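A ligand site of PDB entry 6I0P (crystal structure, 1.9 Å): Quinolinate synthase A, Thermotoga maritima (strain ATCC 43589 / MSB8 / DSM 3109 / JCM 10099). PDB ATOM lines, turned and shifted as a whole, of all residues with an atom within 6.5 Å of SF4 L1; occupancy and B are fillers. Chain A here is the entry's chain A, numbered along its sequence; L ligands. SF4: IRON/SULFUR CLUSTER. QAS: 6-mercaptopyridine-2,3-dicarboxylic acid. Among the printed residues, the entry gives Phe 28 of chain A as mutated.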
ATOM      1  N   HIS A  26     -10.004 -28.709  15.500  1.00  0.00           N
ATOM      2  CA  HIS A  26     -11.308 -28.043  15.580  1.00  0.00           C
ATOM      3  C   HIS A  26     -12.260 -28.646  14.535  1.00  0.00           C
ATOM      4  O   HIS A  26     -11.824 -29.171  13.488  1.00  0.00           O
ATOM      5  CB  HIS A  26     -11.156 -26.537  15.383  1.00  0.00           C
ATOM      6  CG  HIS A  26     -12.401 -25.798  15.706  1.00  0.00           C
ATOM      7  ND1 HIS A  26     -13.338 -25.459  14.740  1.00  0.00           N
ATOM      8  CD2 HIS A  26     -12.864 -25.322  16.878  1.00  0.00           C
ATOM      9  CE1 HIS A  26     -14.330 -24.823  15.302  1.00  0.00           C
ATOM     10  NE2 HIS A  26     -14.072 -24.715  16.624  1.00  0.00           N
ATOM     11  N   PHE A  28     -13.891 -27.198  12.423  1.00  0.00           N
ATOM     12  CA  PHE A  28     -13.878 -26.487  11.114  1.00  0.00           C
ATOM     13  C   PHE A  28     -12.627 -26.838  10.309  1.00  0.00           C
ATOM     14  O   PHE A  28     -12.378 -26.246   9.272  1.00  0.00           O
ATOM     15  CB  PHE A  28     -14.027 -24.984  11.287  1.00  0.00           C
ATOM     16  CG  PHE A  28     -15.338 -24.519  11.891  1.00  0.00           C
ATOM     17  CD1 PHE A  28     -16.417 -25.374  12.056  1.00  0.00           C
ATOM     18  CD2 PHE A  28     -15.470 -23.209  12.310  1.00  0.00           C
ATOM     19  CE1 PHE A  28     -17.602 -24.913  12.608  1.00  0.00           C
ATOM     20  CE2 PHE A  28     -16.647 -22.738  12.867  1.00  0.00           C
ATOM     21  CZ  PHE A  28     -17.725 -23.603  13.031  1.00  0.00           C
ATOM     22  N   VAL A  63      -7.293 -22.191  14.876  1.00  0.00           N
ATOM     23  CA  VAL A  63      -6.766 -20.822  14.713  1.00  0.00           C
ATOM     24  C   VAL A  63      -6.175 -20.387  16.049  1.00  0.00           C
ATOM     25  O   VAL A  63      -6.428 -21.049  17.072  1.00  0.00           O
ATOM     26  CB  VAL A  63      -7.849 -19.832  14.236  1.00  0.00           C
ATOM     27  CG1 VAL A  63      -8.293 -20.151  12.799  1.00  0.00           C
ATOM     28  CG2 VAL A  63      -8.997 -19.788  15.206  1.00  0.00           C
ATOM     29  N   PHE A  65      -6.310 -18.151  18.556  1.00  0.00           N
ATOM     30  CA  PHE A  65      -6.895 -17.869  19.894  1.00  0.00           C
ATOM     31  C   PHE A  65      -7.183 -19.206  20.572  1.00  0.00           C
ATOM     32  O   PHE A  65      -7.138 -19.253  21.788  1.00  0.00           O
ATOM     33  CB  PHE A  65      -8.114 -16.935  19.837  1.00  0.00           C
ATOM     34  CG  PHE A  65      -9.396 -17.568  19.358  1.00  0.00           C
ATOM     35  CD1 PHE A  65     -10.149 -18.387  20.203  1.00  0.00           C
ATOM     36  CD2 PHE A  65      -9.852 -17.372  18.070  1.00  0.00           C
ATOM     37  CE1 PHE A  65     -11.316 -18.997  19.761  1.00  0.00           C
ATOM     38  CE2 PHE A  65     -11.013 -18.000  17.617  1.00  0.00           C
ATOM     39  CZ  PHE A  65     -11.750 -18.799  18.473  1.00  0.00           C
ATOM     40  N   MET A  66      -7.493 -20.240  19.797  1.00  0.00           N
ATOM     41  CA  MET A  66      -7.863 -21.573  20.323  1.00  0.00           C
ATOM     42  C   MET A  66      -6.625 -22.315  20.771  1.00  0.00           C
ATOM     43  O   MET A  66      -6.668 -22.964  21.819  1.00  0.00           O
ATOM     44  CB  MET A  66      -8.524 -22.455  19.259  1.00  0.00           C
ATOM     45  CG  MET A  66      -9.658 -21.854  18.556  1.00  0.00           C
ATOM     46  SD  MET A  66     -10.370 -23.014  17.352  1.00  0.00           S
ATOM     47  CE  MET A  66     -11.833 -22.029  16.994  1.00  0.00           C
ATOM     48  N   THR A  87      -5.856 -17.288  12.183  1.00  0.00           N
ATOM     49  CA  THR A  87      -6.394 -16.349  13.174  1.00  0.00           C
ATOM     50  C   THR A  87      -7.887 -16.157  12.902  1.00  0.00           C
ATOM     51  O   THR A  87      -8.402 -16.616  11.867  1.00  0.00           O
ATOM     52  CB  THR A  87      -5.630 -15.018  13.050  1.00  0.00           C
ATOM     53  OG1 THR A  87      -5.800 -14.227  14.227  1.00  0.00           O
ATOM     54  CG2 THR A  87      -6.006 -14.262  11.785  1.00  0.00           C
ATOM     55  N   CYS A  88      -8.557 -15.426  13.782  1.00  0.00           N
ATOM     56  CA  CYS A  88      -9.975 -15.094  13.649  1.00  0.00           C
ATOM     57  C   CYS A  88     -10.106 -13.593  13.393  1.00  0.00           C
ATOM     58  O   CYS A  88      -9.831 -12.778  14.271  1.00  0.00           O
ATOM     59  CB  CYS A  88     -10.710 -15.541  14.903  1.00  0.00           C
ATOM     60  SG  CYS A  88     -12.448 -15.008  14.965  1.00  0.00           S
ATOM     61  N   PRO A  89     -10.465 -13.155  12.171  1.00  0.00           N
ATOM     62  CA  PRO A  89     -10.562 -11.730  11.896  1.00  0.00           C
ATOM     63  C   PRO A  89     -11.543 -11.033  12.845  1.00  0.00           C
ATOM     64  O   PRO A  89     -11.277  -9.932  13.251  1.00  0.00           O
ATOM     65  CB  PRO A  89     -11.011 -11.703  10.437  1.00  0.00           C
ATOM     66  CG  PRO A  89     -10.490 -13.015   9.881  1.00  0.00           C
ATOM     67  CD  PRO A  89     -10.748 -14.002  10.992  1.00  0.00           C
ATOM     68  N   MET A  90     -12.632 -11.692  13.207  1.00  0.00           N
ATOM     69  CA  MET A  90     -13.652 -11.125  14.126  1.00  0.00           C
ATOM     70  C   MET A  90     -13.018 -10.883  15.495  1.00  0.00           C
ATOM     71  O   MET A  90     -13.246  -9.824  16.072  1.00  0.00           O
ATOM     72  CB  MET A  90     -14.846 -12.062  14.301  1.00  0.00           C
ATOM     73  CG  MET A  90     -15.858 -11.525  15.297  1.00  0.00           C
ATOM     74  SD  MET A  90     -17.170 -12.703  15.699  1.00  0.00           S
ATOM     75  CE  MET A  90     -16.252 -14.006  16.525  1.00  0.00           C
ATOM     76  N   ALA A  91     -12.281 -11.867  16.020  1.00  0.00           N
ATOM     77  CA  ALA A  91     -11.624 -11.705  17.319  1.00  0.00           C
ATOM     78  C   ALA A  91     -10.732 -10.459  17.232  1.00  0.00           C
ATOM     79  O   ALA A  91     -10.676  -9.649  18.172  1.00  0.00           O
ATOM     80  CB  ALA A  91     -10.839 -12.957  17.686  1.00  0.00           C
ATOM     81  N   TYR A 114     -16.638 -13.461  24.531  1.00  0.00           N
ATOM     82  CA  TYR A 114     -16.782 -14.719  23.786  1.00  0.00           C
ATOM     83  C   TYR A 114     -15.368 -15.310  23.660  1.00  0.00           C
ATOM     84  O   TYR A 114     -14.377 -14.580  23.475  1.00  0.00           O
ATOM     85  CB  TYR A 114     -17.457 -14.374  22.464  1.00  0.00           C
ATOM     86  CG  TYR A 114     -17.768 -15.529  21.533  1.00  0.00           C
ATOM     87  CD1 TYR A 114     -18.137 -16.767  22.031  1.00  0.00           C
ATOM     88  CD2 TYR A 114     -17.745 -15.336  20.172  1.00  0.00           C
ATOM     89  CE1 TYR A 114     -18.442 -17.811  21.177  1.00  0.00           C
ATOM     90  CE2 TYR A 114     -18.051 -16.377  19.297  1.00  0.00           C
ATOM     91  CZ  TYR A 114     -18.392 -17.615  19.808  1.00  0.00           C
ATOM     92  OH  TYR A 114     -18.692 -18.673  18.989  1.00  0.00           O
ATOM     93  N   ASN A 116     -14.013 -16.564  21.335  1.00  0.00           N
ATOM     94  CA  ASN A 116     -13.458 -16.116  20.040  1.00  0.00           C
ATOM     95  C   ASN A 116     -13.011 -14.668  20.222  1.00  0.00           C
ATOM     96  O   ASN A 116     -13.782 -13.695  19.904  1.00  0.00           O
ATOM     97  CB  ASN A 116     -14.464 -16.284  18.886  1.00  0.00           C
ATOM     98  CG  ASN A 116     -14.981 -17.702  18.664  1.00  0.00           C
ATOM     99  OD1 ASN A 116     -15.065 -18.520  19.596  1.00  0.00           O
ATOM    100  ND2 ASN A 116     -15.360 -18.024  17.438  1.00  0.00           N
ATOM    101  N   ASP A 151     -18.803 -10.587  19.215  1.00  0.00           N
ATOM    102  CA  ASP A 151     -19.817 -10.969  18.223  1.00  0.00           C
ATOM    103  C   ASP A 151     -21.141 -10.303  18.597  1.00  0.00           C
ATOM    104  O   ASP A 151     -21.738 -10.647  19.609  1.00  0.00           O
ATOM    105  CB  ASP A 151     -19.937 -12.477  18.076  1.00  0.00           C
ATOM    106  CG  ASP A 151     -20.813 -12.864  16.891  1.00  0.00           C
ATOM    107  OD1 ASP A 151     -22.010 -12.473  16.897  1.00  0.00           O
ATOM    108  OD2 ASP A 151     -20.285 -13.454  15.933  1.00  0.00           O
ATOM    109  N   HIS A 174     -18.912  -9.192  13.987  1.00  0.00           N
ATOM    110  CA  HIS A 174     -19.632 -10.350  13.442  1.00  0.00           C
ATOM    111  C   HIS A 174     -18.657 -11.343  12.811  1.00  0.00           C
ATOM    112  O   HIS A 174     -17.486 -10.969  12.518  1.00  0.00           O
ATOM    113  CB  HIS A 174     -20.660  -9.888  12.408  1.00  0.00           C
ATOM    114  CG  HIS A 174     -19.994  -9.410  11.181  1.00  0.00           C
ATOM    115  ND1 HIS A 174     -19.248  -8.246  11.167  1.00  0.00           N
ATOM    116  CD2 HIS A 174     -19.871  -9.966   9.955  1.00  0.00           C
ATOM    117  CE1 HIS A 174     -18.714  -8.086   9.969  1.00  0.00           C
ATOM    118  NE2 HIS A 174     -19.087  -9.117   9.209  1.00  0.00           N
ATOM    119  N   CYS A 175     -19.146 -12.553  12.570  1.00  0.00           N
ATOM    120  CA  CYS A 175     -18.402 -13.619  11.893  1.00  0.00           C
ATOM    121  C   CYS A 175     -18.921 -13.733  10.466  1.00  0.00           C
ATOM    122  O   CYS A 175     -20.078 -14.095  10.296  1.00  0.00           O
ATOM    123  CB  CYS A 175     -18.592 -14.942  12.598  1.00  0.00           C
ATOM    124  SG  CYS A 175     -18.020 -16.319  11.571  1.00  0.00           S
ATOM    125  N   PRO A 176     -18.109 -13.440   9.425  1.00  0.00           N
ATOM    126  CA  PRO A 176     -18.567 -13.412   8.030  1.00  0.00           C
ATOM    127  C   PRO A 176     -19.090 -14.780   7.589  1.00  0.00           C
ATOM    128  O   PRO A 176     -19.985 -14.895   6.779  1.00  0.00           O
ATOM    129  CB  PRO A 176     -17.319 -13.053   7.210  1.00  0.00           C
ATOM    130  CG  PRO A 176     -16.397 -12.415   8.202  1.00  0.00           C
ATOM    131  CD  PRO A 176     -16.694 -13.062   9.543  1.00  0.00           C
ATOM    132  N   VAL A 177     -18.540 -15.828   8.181  1.00  0.00           N
ATOM    133  CA  VAL A 177     -18.862 -17.223   7.832  1.00  0.00           C
ATOM    134  C   VAL A 177     -20.344 -17.523   8.145  1.00  0.00           C
ATOM    135  O   VAL A 177     -20.971 -18.285   7.420  1.00  0.00           O
ATOM    136  CB  VAL A 177     -17.918 -18.189   8.572  1.00  0.00           C
ATOM    137  CG1 VAL A 177     -18.331 -19.620   8.364  1.00  0.00           C
ATOM    138  CG2 VAL A 177     -16.469 -18.004   8.190  1.00  0.00           C
ATOM    139  N   HIS A 178     -20.919 -16.895   9.177  1.00  0.00           N
ATOM    140  CA  HIS A 178     -22.284 -17.233   9.618  1.00  0.00           C
ATOM    141  C   HIS A 178     -23.335 -16.252   9.076  1.00  0.00           C
ATOM    142  O   HIS A 178     -24.473 -16.333   9.547  1.00  0.00           O
ATOM    143  CB  HIS A 178     -22.328 -17.310  11.156  1.00  0.00           C
ATOM    144  CG  HIS A 178     -21.691 -18.545  11.690  1.00  0.00           C
ATOM    145  ND1 HIS A 178     -20.356 -18.597  12.033  1.00  0.00           N
ATOM    146  CD2 HIS A 178     -22.156 -19.802  11.813  1.00  0.00           C
ATOM    147  CE1 HIS A 178     -20.052 -19.847  12.404  1.00  0.00           C
ATOM    148  NE2 HIS A 178     -21.132 -20.605  12.293  1.00  0.00           N
ATOM    149  N   GLU A 202     -24.295 -17.159  16.243  1.00  0.00           N
ATOM    150  CA  GLU A 202     -23.600 -16.103  15.489  1.00  0.00           C
ATOM    151  C   GLU A 202     -24.343 -15.746  14.192  1.00  0.00           C
ATOM    152  O   GLU A 202     -23.942 -14.758  13.543  1.00  0.00           O
ATOM    153  CB  GLU A 202     -22.166 -16.506  15.179  1.00  0.00           C
ATOM    154  CG  GLU A 202     -21.297 -16.474  16.435  1.00  0.00           C
ATOM    155  CD  GLU A 202     -19.818 -16.753  16.213  1.00  0.00           C
ATOM    156  OE1 GLU A 202     -19.076 -15.796  15.846  1.00  0.00           O
ATOM    157  OE2 GLU A 202     -19.419 -17.921  16.408  1.00  0.00           O
ATOM    158  N   GLU A 237     -20.126 -23.498   9.611  1.00  0.00           N
ATOM    159  CA  GLU A 237     -18.979 -23.684   8.717  1.00  0.00           C
ATOM    160  C   GLU A 237     -18.983 -25.149   8.240  1.00  0.00           C
ATOM    161  O   GLU A 237     -19.396 -26.032   9.003  1.00  0.00           O
ATOM    162  CB  GLU A 237     -17.693 -23.299   9.470  1.00  0.00           C
ATOM    163  CG  GLU A 237     -16.535 -22.888   8.582  1.00  0.00           C
ATOM    164  CD  GLU A 237     -15.704 -23.980   7.999  1.00  0.00           C
ATOM    165  OE1 GLU A 237     -15.858 -25.161   8.420  1.00  0.00           O
ATOM    166  OE2 GLU A 237     -14.854 -23.642   7.175  1.00  0.00           O
ATOM    167  N   CYS A 261     -14.487 -20.948   6.386  1.00  0.00           N
ATOM    168  CA  CYS A 261     -13.601 -20.049   7.146  1.00  0.00           C
ATOM    169  C   CYS A 261     -12.205 -20.172   6.540  1.00  0.00           C
ATOM    170  O   CYS A 261     -11.562 -21.252   6.666  1.00  0.00           O
ATOM    171  CB  CYS A 261     -13.601 -20.339   8.646  1.00  0.00           C
ATOM    172  SG  CYS A 261     -12.447 -19.254   9.534  1.00  0.00           S
ATOM    173  N   VAL A 262     -11.761 -19.107   5.869  1.00  0.00           N
ATOM    174  CA  VAL A 262     -10.491 -19.142   5.127  1.00  0.00           C
ATOM    175  C   VAL A 262      -9.347 -19.435   6.101  1.00  0.00           C
ATOM    176  O   VAL A 262      -8.474 -20.233   5.768  1.00  0.00           O
ATOM    177  CB  VAL A 262     -10.249 -17.869   4.293  1.00  0.00           C
ATOM    178  CG1 VAL A 262      -8.845 -17.857   3.736  1.00  0.00           C
ATOM    179  CG2 VAL A 262     -11.266 -17.767   3.157  1.00  0.00           C
ATOM    180  N   ASN A 263      -9.368 -18.823   7.273  1.00  0.00           N
ATOM    181  CA  ASN A 263      -8.314 -19.055   8.270  1.00  0.00           C
ATOM    182  C   ASN A 263      -8.262 -20.509   8.732  1.00  0.00           C
ATOM    183  O   ASN A 263      -7.169 -21.097   8.855  1.00  0.00           O
ATOM    184  CB  ASN A 263      -8.463 -18.076   9.421  1.00  0.00           C
ATOM    185  CG  ASN A 263      -7.668 -16.817   9.166  1.00  0.00           C
ATOM    186  OD1 ASN A 263      -6.456 -16.806   9.348  1.00  0.00           O
ATOM    187  ND2 ASN A 263      -8.343 -15.758   8.718  1.00  0.00           N
ATOM    188  N   MET A 264      -9.426 -21.128   8.974  1.00  0.00           N
ATOM    189  CA  MET A 264      -9.486 -22.548   9.344  1.00  0.00           C
ATOM    190  C   MET A 264      -8.888 -23.405   8.227  1.00  0.00           C
ATOM    191  O   MET A 264      -8.234 -24.437   8.535  1.00  0.00           O
ATOM    192  CB  MET A 264     -10.930 -22.972   9.631  1.00  0.00           C
ATOM    193  CG  MET A 264     -11.441 -22.442  10.969  1.00  0.00           C
ATOM    194  SD  MET A 264     -10.645 -23.344  12.288  1.00  0.00           S
ATOM    195  CE  MET A 264     -11.490 -22.618  13.712  1.00  0.00           C
HETATM  196 FE1  SF4 L   1     -15.975 -17.032  12.279  1.00  0.00          FE
HETATM  197 FE2  SF4 L   1     -13.404 -18.311  11.390  1.00  0.00          FE
HETATM  198 FE3  SF4 L   1     -14.734 -18.943  13.764  1.00  0.00          FE
HETATM  199 FE4  SF4 L   1     -13.506 -16.298  13.471  1.00  0.00          FE
HETATM  200  S1  SF4 L   1     -12.400 -18.371  13.426  1.00  0.00           S
HETATM  201  S2  SF4 L   1     -15.700 -16.994  14.440  1.00  0.00           S
HETATM  202  S3  SF4 L   1     -14.067 -15.952  11.293  1.00  0.00           S
HETATM  203  S4  SF4 L   1     -15.583 -19.307  11.742  1.00  0.00           S
HETATM  204  O1  QAS L   2     -16.746 -22.945  20.074  1.00  0.00           O
HETATM  205  C7  QAS L   2     -16.032 -23.231  19.066  1.00  0.00           C
HETATM  206  O2  QAS L   2     -15.056 -23.994  19.070  1.00  0.00           O
HETATM  207  C2  QAS L   2     -16.440 -22.506  17.870  1.00  0.00           C
HETATM  208  N1  QAS L   2     -15.502 -21.851  17.221  1.00  0.00           N
HETATM  209  C6  QAS L   2     -15.750 -21.101  16.152  1.00  0.00           C
HETATM  210  S   QAS L   2     -14.329 -20.471  15.450  1.00  0.00           S
HETATM  211  C5  QAS L   2     -17.028 -20.931  15.643  1.00  0.00           C
HETATM  212  C4  QAS L   2     -18.076 -21.615  16.290  1.00  0.00           C
HETATM  213  C3  QAS L   2     -17.821 -22.392  17.414  1.00  0.00           C
HETATM  214  C8  QAS L   2     -18.852 -23.242  18.098  1.00  0.00           C
HETATM  215  O4  QAS L   2     -20.066 -23.053  17.938  1.00  0.00           O
HETATM  216  O3  QAS L   2     -18.418 -24.363  18.565  1.00  0.00           O
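The side-chain sulfur (SG) of Cys 88 binds an iron atom (FE4) of SF4 L1.
The side-chain sulfur (SG) of Cys 175 is bound to an iron atom (FE1) of SF4 L1 (2.3 Å).
SG of Cys 261 binds FE2 of SF4 L1, at 2.3 Å.
A sulfur (S2) of SF4 L1 lies close to the side-chain amide nitrogen (ND2) of Asn 116 (3.2 Å).
A sulfur (S) of QAS L2 lies close to the side-chain amide nitrogen of Asn 116 (3.3 Å).
A ring nitrogen (NE2) of His 26 is in hydrogen-bond range of an oxygen (O2) of QAS L2, 2.7 Å away.
S of QAS L2 is bound to FE3 of SF4 L1 (2.3 Å).
The side-chain sulfur of Cys 88 sits close to the backbone NH of Met 90 (3.8 Å).
The side-chain sulfur (SG) of Cys 88 sits close to the backbone NH (N) of Ala 91, 3.3 Å away.
The backbone NH of Cys 175 lies within hydrogen-bond range of the side-chain sulfur of Met 90, 3.7 Å away.
SG of Cys 175 sits close to N of Val 177, 3.5 Å away.
The side-chain sulfur (SG) of Cys 175 sits close to a ring nitrogen (ND1) of His 178, at 3.3 Å.
The backbone NH (N) of Met 264 sits close to the side-chain sulfur (SG) of Cys 261 (3.6 Å).
The backbone NH (N) of Phe 28 sits at hydrogen-bond distance from a ring nitrogen (ND1) of His 26 (2.9 Å).
OD2 of Asp 151 sits close to OE1 of Glu 202 (2.6 Å).
Phe 28 touches SF4 L1 (CE2 to S4, 3.8 Å).
Pro 89 touches SF4 L1.
Met 90 touches SF4 L1.
Val 177 touches SF4 L1.
OE1 of Glu 202 touches S2 of SF4 L1, 3.8 Å away.
Hydrophobic or aromatic side chains that line SF4 L1: Phe 28, Pro 89, Met 90 and Val 177.
The nearest printed residue that does not touch SF4 L1 is Val 63 (4.1 Å).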
